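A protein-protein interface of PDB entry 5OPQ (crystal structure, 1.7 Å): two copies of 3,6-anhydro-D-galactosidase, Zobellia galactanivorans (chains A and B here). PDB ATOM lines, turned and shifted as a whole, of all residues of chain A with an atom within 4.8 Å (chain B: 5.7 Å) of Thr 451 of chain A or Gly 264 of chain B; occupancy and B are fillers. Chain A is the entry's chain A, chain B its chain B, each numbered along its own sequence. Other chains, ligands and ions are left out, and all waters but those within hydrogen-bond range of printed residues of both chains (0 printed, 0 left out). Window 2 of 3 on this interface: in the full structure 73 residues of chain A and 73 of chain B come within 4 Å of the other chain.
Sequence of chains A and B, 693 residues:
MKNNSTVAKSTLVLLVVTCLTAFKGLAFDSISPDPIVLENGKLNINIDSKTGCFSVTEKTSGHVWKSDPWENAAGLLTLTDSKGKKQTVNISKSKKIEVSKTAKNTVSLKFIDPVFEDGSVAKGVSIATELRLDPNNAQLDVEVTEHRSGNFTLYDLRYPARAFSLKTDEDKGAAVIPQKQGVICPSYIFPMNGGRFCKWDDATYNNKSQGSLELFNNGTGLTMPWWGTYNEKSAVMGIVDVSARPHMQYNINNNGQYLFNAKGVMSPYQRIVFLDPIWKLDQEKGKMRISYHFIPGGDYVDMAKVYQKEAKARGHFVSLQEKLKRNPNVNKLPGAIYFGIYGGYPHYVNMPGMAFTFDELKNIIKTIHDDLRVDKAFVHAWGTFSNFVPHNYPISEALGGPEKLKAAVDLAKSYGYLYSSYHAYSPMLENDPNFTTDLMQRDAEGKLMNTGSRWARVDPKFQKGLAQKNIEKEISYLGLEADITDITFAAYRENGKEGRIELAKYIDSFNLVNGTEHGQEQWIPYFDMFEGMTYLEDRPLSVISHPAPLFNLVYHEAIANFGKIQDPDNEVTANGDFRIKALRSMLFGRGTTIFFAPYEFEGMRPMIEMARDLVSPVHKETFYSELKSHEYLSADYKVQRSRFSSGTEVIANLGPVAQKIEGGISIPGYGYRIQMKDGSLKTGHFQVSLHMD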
ATOM      1  N   MET A 440       0.083 -14.944 -13.288  1.00  0.00           N
ATOM      2  CA  MET A 440       1.241 -15.392 -12.573  1.00  0.00           C
ATOM      3  C   MET A 440       2.161 -16.218 -13.436  1.00  0.00           C
ATOM      4  O   MET A 440       1.666 -16.984 -14.311  1.00  0.00           O
ATOM      5  CB  MET A 440       0.858 -16.114 -11.285  1.00  0.00           C
ATOM      6  CG  MET A 440       0.130 -15.221 -10.323  1.00  0.00           C
ATOM      7  SD  MET A 440      -0.417 -16.033  -8.824  1.00  0.00           S
ATOM      8  CE  MET A 440       1.120 -16.586  -8.121  1.00  0.00           C
ATOM      9  N   LYS A 447       4.663 -25.058 -12.113  1.00  0.00           N
ATOM     10  CA  LYS A 447       4.293 -24.601 -10.764  1.00  0.00           C
ATOM     11  C   LYS A 447       4.320 -23.096 -10.732  1.00  0.00           C
ATOM     12  O   LYS A 447       5.180 -22.479 -11.363  1.00  0.00           O
ATOM     13  CB  LYS A 447       5.317 -25.159  -9.819  1.00  0.00           C
ATOM     14  CG  LYS A 447       5.254 -26.669  -9.760  1.00  0.00           C
ATOM     15  CD  LYS A 447       5.971 -27.264  -8.546  1.00  0.00           C
ATOM     16  CE  LYS A 447       6.893 -26.298  -7.906  1.00  0.00           C
ATOM     17  NZ  LYS A 447       7.947 -27.038  -7.194  1.00  0.00           N
ATOM     18  N   LEU A 448       3.444 -22.517  -9.924  1.00  0.00           N
ATOM     19  CA  LEU A 448       3.380 -21.059  -9.784  1.00  0.00           C
ATOM     20  C   LEU A 448       4.661 -20.553  -9.144  1.00  0.00           C
ATOM     21  O   LEU A 448       5.152 -21.159  -8.188  1.00  0.00           O
ATOM     22  CB  LEU A 448       2.134 -20.614  -9.006  1.00  0.00           C
ATOM     23  CG  LEU A 448       0.782 -20.870  -9.629  1.00  0.00           C
ATOM     24  CD1 LEU A 448      -0.290 -20.750  -8.570  1.00  0.00           C
ATOM     25  CD2 LEU A 448       0.625 -19.905 -10.774  1.00  0.00           C
ATOM     26  N   MET A 449       5.133 -19.430  -9.638  1.00  0.00           N
ATOM     27  CA  MET A 449       6.216 -18.674  -9.081  1.00  0.00           C
ATOM     28  C   MET A 449       5.641 -17.510  -8.197  1.00  0.00           C
ATOM     29  O   MET A 449       4.574 -16.976  -8.430  1.00  0.00           O
ATOM     30  CB  MET A 449       7.148 -18.162 -10.167  1.00  0.00           C
ATOM     31  CG  MET A 449       7.796 -19.307 -10.941  1.00  0.00           C
ATOM     32  SD  MET A 449       8.569 -18.782 -12.426  1.00  0.00           S
ATOM     33  CE  MET A 449       9.809 -17.641 -11.862  1.00  0.00           C
ATOM     34  N   ASN A 450       6.380 -17.135  -7.168  1.00  0.00           N
ATOM     35  CA  ASN A 450       5.975 -16.047  -6.314  1.00  0.00           C
ATOM     36  C   ASN A 450       4.705 -16.207  -5.525  1.00  0.00           C
ATOM     37  O   ASN A 450       4.015 -15.232  -5.145  1.00  0.00           O
ATOM     38  CB  ASN A 450       5.937 -14.745  -7.071  1.00  0.00           C
ATOM     39  CG  ASN A 450       7.141 -14.504  -7.819  1.00  0.00           C
ATOM     40  OD1 ASN A 450       7.131 -14.491  -9.091  1.00  0.00           O
ATOM     41  ND2 ASN A 450       8.197 -14.291  -7.111  1.00  0.00           N
ATOM     42  N   THR A 451       4.424 -17.431  -5.162  1.00  0.00           N
ATOM     43  CA  THR A 451       3.319 -17.723  -4.340  1.00  0.00           C
ATOM     44  C   THR A 451       3.605 -17.090  -2.947  1.00  0.00           C
ATOM     45  O   THR A 451       2.683 -16.757  -2.235  1.00  0.00           O
ATOM     46  CB  THR A 451       3.012 -19.207  -4.142  1.00  0.00           C
ATOM     47  OG1 THR A 451       4.175 -19.938  -3.767  1.00  0.00           O
ATOM     48  CG2 THR A 451       2.417 -19.783  -5.462  1.00  0.00           C
ATOM     49  N   GLY A 452       4.832 -16.905  -2.681  1.00  0.00           N
ATOM     50  CA  GLY A 452       5.182 -16.305  -1.303  1.00  0.00           C
ATOM     51  C   GLY A 452       5.334 -14.818  -1.317  1.00  0.00           C
ATOM     52  O   GLY A 452       5.637 -14.238  -0.224  1.00  0.00           O
ATOM     53  N   SER A 453       5.179 -14.144  -2.498  1.00  0.00           N
ATOM     54  CA  SER A 453       5.474 -12.678  -2.621  1.00  0.00           C
ATOM     55  C   SER A 453       4.305 -12.012  -3.300  1.00  0.00           C
ATOM     56  O   SER A 453       4.370 -11.732  -4.482  1.00  0.00           O
ATOM     57  CB  SER A 453       6.735 -12.291  -3.364  1.00  0.00           C
ATOM     58  OG  SER A 453       7.787 -12.909  -2.734  1.00  0.00           O
ATOM     59  N   ARG A 457       3.679 -10.678  -8.092  1.00  0.00           N
ATOM     60  CA  ARG A 457       3.062 -11.919  -8.644  1.00  0.00           C
ATOM     61  C   ARG A 457       2.781 -11.838 -10.141  1.00  0.00           C
ATOM     62  O   ARG A 457       2.836 -12.908 -10.806  1.00  0.00           O
ATOM     63  CB  ARG A 457       1.874 -12.427  -7.966  1.00  0.00           C
ATOM     64  CG  ARG A 457       2.154 -13.037  -6.645  1.00  0.00           C
ATOM     65  CD  ARG A 457       0.946 -13.440  -5.938  1.00  0.00           C
ATOM     66  NE  ARG A 457       1.193 -14.197  -4.703  1.00  0.00           N
ATOM     67  CZ  ARG A 457       0.380 -14.179  -3.644  1.00  0.00           C
ATOM     68  NH1 ARG A 457      -0.717 -13.472  -3.651  1.00  0.00           N
ATOM     69  NH2 ARG A 457       0.738 -14.781  -2.536  1.00  0.00           N
ATOM     70  N   GLN B 257       0.353 -20.256   3.669  1.00  0.00           N
ATOM     71  CA  GLN B 257       1.006 -20.240   2.394  1.00  0.00           C
ATOM     72  C   GLN B 257       2.393 -20.828   2.458  1.00  0.00           C
ATOM     73  O   GLN B 257       2.830 -21.495   1.534  1.00  0.00           O
ATOM     74  CB  GLN B 257       1.058 -18.803   1.822  1.00  0.00           C
ATOM     75  CG  GLN B 257       1.632 -18.664   0.422  1.00  0.00           C
ATOM     76  CD  GLN B 257       0.816 -19.528  -0.562  1.00  0.00           C
ATOM     77  OE1 GLN B 257      -0.434 -19.330  -0.706  1.00  0.00           O
ATOM     78  NE2 GLN B 257       1.529 -20.412  -1.287  1.00  0.00           N
ATOM     79  N   PHE B 260       2.789 -24.317   1.293  1.00  0.00           N
ATOM     80  CA  PHE B 260       2.501 -24.605  -0.127  1.00  0.00           C
ATOM     81  C   PHE B 260       3.487 -23.985  -1.121  1.00  0.00           C
ATOM     82  O   PHE B 260       3.376 -24.199  -2.321  1.00  0.00           O
ATOM     83  CB  PHE B 260       1.089 -24.110  -0.384  1.00  0.00           C
ATOM     84  CG  PHE B 260       0.054 -24.876   0.326  1.00  0.00           C
ATOM     85  CD1 PHE B 260      -0.392 -26.131  -0.189  1.00  0.00           C
ATOM     86  CD2 PHE B 260      -0.494 -24.426   1.498  1.00  0.00           C
ATOM     87  CE1 PHE B 260      -1.362 -26.835   0.524  1.00  0.00           C
ATOM     88  CE2 PHE B 260      -1.448 -25.138   2.190  1.00  0.00           C
ATOM     89  CZ  PHE B 260      -1.865 -26.342   1.709  1.00  0.00           C
ATOM     90  N   ASN B 261       4.390 -23.104  -0.673  1.00  0.00           N
ATOM     91  CA  ASN B 261       5.286 -22.472  -1.599  1.00  0.00           C
ATOM     92  C   ASN B 261       6.153 -23.422  -2.411  1.00  0.00           C
ATOM     93  O   ASN B 261       6.449 -23.155  -3.596  1.00  0.00           O
ATOM     94  CB  ASN B 261       6.148 -21.483  -0.880  1.00  0.00           C
ATOM     95  CG  ASN B 261       5.345 -20.255  -0.415  1.00  0.00           C
ATOM     96  OD1 ASN B 261       4.393 -19.846  -1.053  1.00  0.00           O
ATOM     97  ND2 ASN B 261       5.770 -19.672   0.709  1.00  0.00           N
ATOM     98  N   ALA B 262       6.659 -24.471  -1.745  1.00  0.00           N
ATOM     99  CA  ALA B 262       7.564 -25.374  -2.463  1.00  0.00           C
ATOM    100  C   ALA B 262       6.768 -26.095  -3.518  1.00  0.00           C
ATOM    101  O   ALA B 262       7.330 -26.410  -4.535  1.00  0.00           O
ATOM    102  CB  ALA B 262       8.220 -26.386  -1.527  1.00  0.00           C
ATOM    103  N   LYS B 263       5.492 -26.343  -3.294  1.00  0.00           N
ATOM    104  CA  LYS B 263       4.625 -26.990  -4.280  1.00  0.00           C
ATOM    105  C   LYS B 263       4.161 -26.040  -5.353  1.00  0.00           C
ATOM    106  O   LYS B 263       3.510 -26.464  -6.320  1.00  0.00           O
ATOM    107  CB  LYS B 263       3.387 -27.578  -3.640  1.00  0.00           C
ATOM    108  CG  LYS B 263       3.595 -28.896  -2.868  1.00  0.00           C
ATOM    109  CD  LYS B 263       2.526 -28.997  -1.791  1.00  0.00           C
ATOM    110  CE  LYS B 263       2.483 -30.324  -1.076  1.00  0.00           C
ATOM    111  NZ  LYS B 263       1.288 -30.204  -0.205  1.00  0.00           N
ATOM    112  N   GLY B 264       4.352 -24.742  -5.175  1.00  0.00           N
ATOM    113  CA  GLY B 264       3.884 -23.772  -6.190  1.00  0.00           C
ATOM    114  C   GLY B 264       2.393 -23.645  -6.339  1.00  0.00           C
ATOM    115  O   GLY B 264       1.872 -23.533  -7.469  1.00  0.00           O
ATOM    116  N   VAL B 265       1.629 -23.780  -5.286  1.00  0.00           N
ATOM    117  CA  VAL B 265       0.201 -23.562  -5.301  1.00  0.00           C
ATOM    118  C   VAL B 265      -0.240 -22.553  -4.233  1.00  0.00           C
ATOM    119  O   VAL B 265       0.560 -22.275  -3.326  1.00  0.00           O
ATOM    120  CB  VAL B 265      -0.636 -24.862  -5.152  1.00  0.00           C
ATOM    121  CG1 VAL B 265      -0.205 -25.954  -6.155  1.00  0.00           C
ATOM    122  CG2 VAL B 265      -0.527 -25.457  -3.762  1.00  0.00           C
ATOM    123  N   MET B 266      -1.428 -21.982  -4.414  1.00  0.00           N
ATOM    124  CA  MET B 266      -1.979 -21.037  -3.450  1.00  0.00           C
ATOM    125  C   MET B 266      -2.540 -21.782  -2.269  1.00  0.00           C
ATOM    126  O   MET B 266      -3.218 -22.771  -2.414  1.00  0.00           O
ATOM    127  CB  MET B 266      -3.056 -20.134  -4.054  1.00  0.00           C
ATOM    128  CG  MET B 266      -2.566 -19.349  -5.265  1.00  0.00           C
ATOM    129  SD  MET B 266      -1.142 -18.280  -4.963  1.00  0.00           S
ATOM    130  CE  MET B 266      -1.868 -17.319  -3.636  1.00  0.00           C
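The side-chain amide oxygen (OD1) of Asn 261 of chain B sits at hydrogen-bond distance from the side-chain hydroxyl (OG1) of Thr 451 of chain A, 2.7 Å away. N of Leu 448 of chain A sits at hydrogen-bond distance from O of Gly 264 of chain B (3.1 Å). NZ of Lys 447 of chain A lies within hydrogen-bond range of O of Ala 262 of chain B (2.8 Å). The side-chain amide oxygen (OD1) of Asn 261 of chain B is in hydrogen-bond range of the backbone NH (N) of Gly 452 of chain A (3.4 Å).
The guanidinium group of Arg 457 of chain A sits at hydrogen-bond distance from the backbone carbonyl oxygen of Thr 451 of chain A. NE2 of Gln 257 of chain B sits at hydrogen-bond distance from OD1 of Asn 261 of chain B, 2.9 Å away. The side-chain amide nitrogen of Gln 257 of chain B is in hydrogen-bond range of the backbone carbonyl oxygen of Val 265 of chain B (2.9 Å). The backbone carbonyl oxygen (O) of Asn 450 of chain A lies within hydrogen-bond range of the guanidinium group (NE) of Arg 457 of chain A, at 3.0 Å. N of Val 265 of chain B is in hydrogen-bond range of O of Phe 260 of chain B (3.5 Å).
Among the printed residues, pairs that only touch across the chains: Lys 447 of chain A with Lys 263 of chain B (3.4 Å), Thr 451 of chain A with Gln 257 of chain B (3.4 Å), Thr 451 of chain A with Gly 264 of chain B (3.96 Å), Thr 451 of chain A with Val 265 of chain B (3.8 Å), Thr 451 of chain A with Met 266 of chain B (3.9 Å) and Arg 457 of chain A with Met 266 of chain B (3.8 Å).
Thr 451 of chain A touches just these residues of chain B: Gln 257, Asn 261, Gly 264, Val 265 and Met 266. Of chain A, only Leu 448 (3.1 Å) and Thr 451 (3.96 Å) come within 4 Å of Gly 264 of chain B. Printed residues of chain B within 4 Å of Gly 452 of chain A: Asn 261 (3.4 Å). Of the printed residues of chain B, Lys 447 of chain A touches Ala 262 and Lys 263. Of the printed residues of chain A, Met 266 of chain B touches Thr 451 (3.9 Å) and Arg 457 (3.8 Å). Of the printed residues of chain A, Ala 262 of chain B touches Lys 447 (2.8 Å). Printed residues of chain B within 4 Å of Arg 457 of chain A: Met 266 (3.8 Å). The nearest residue of chain A that does not touch Gly 264 of chain B is Lys 447 of chain A (4.04 Å).
Of the 8 printed residues of chain B, 7 touch a printed residue of chain A. Hydrophobic or aromatic side chains of chain B that line the printed part of chain A: Met 266. Of the 9 printed residues of chain A, 5 touch a printed residue of chain B. Hydrophobic or aromatic side chains of chain A that line the printed part of chain B: Leu 448. Along chain A the printed residues that touch a printed residue of chain B span positions 447 to 457. Among the printed residues, 10 pairs touch across the chains. Among the printed residues, no Asp or Glu carboxylate lies within 4 Å of a Lys or Arg side-chain nitrogen of the other chain.
No position is printed for both chains. Of the 10 pairs that touch across the chains among the printed residues, none has its exchanged pair printed and touching as well.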
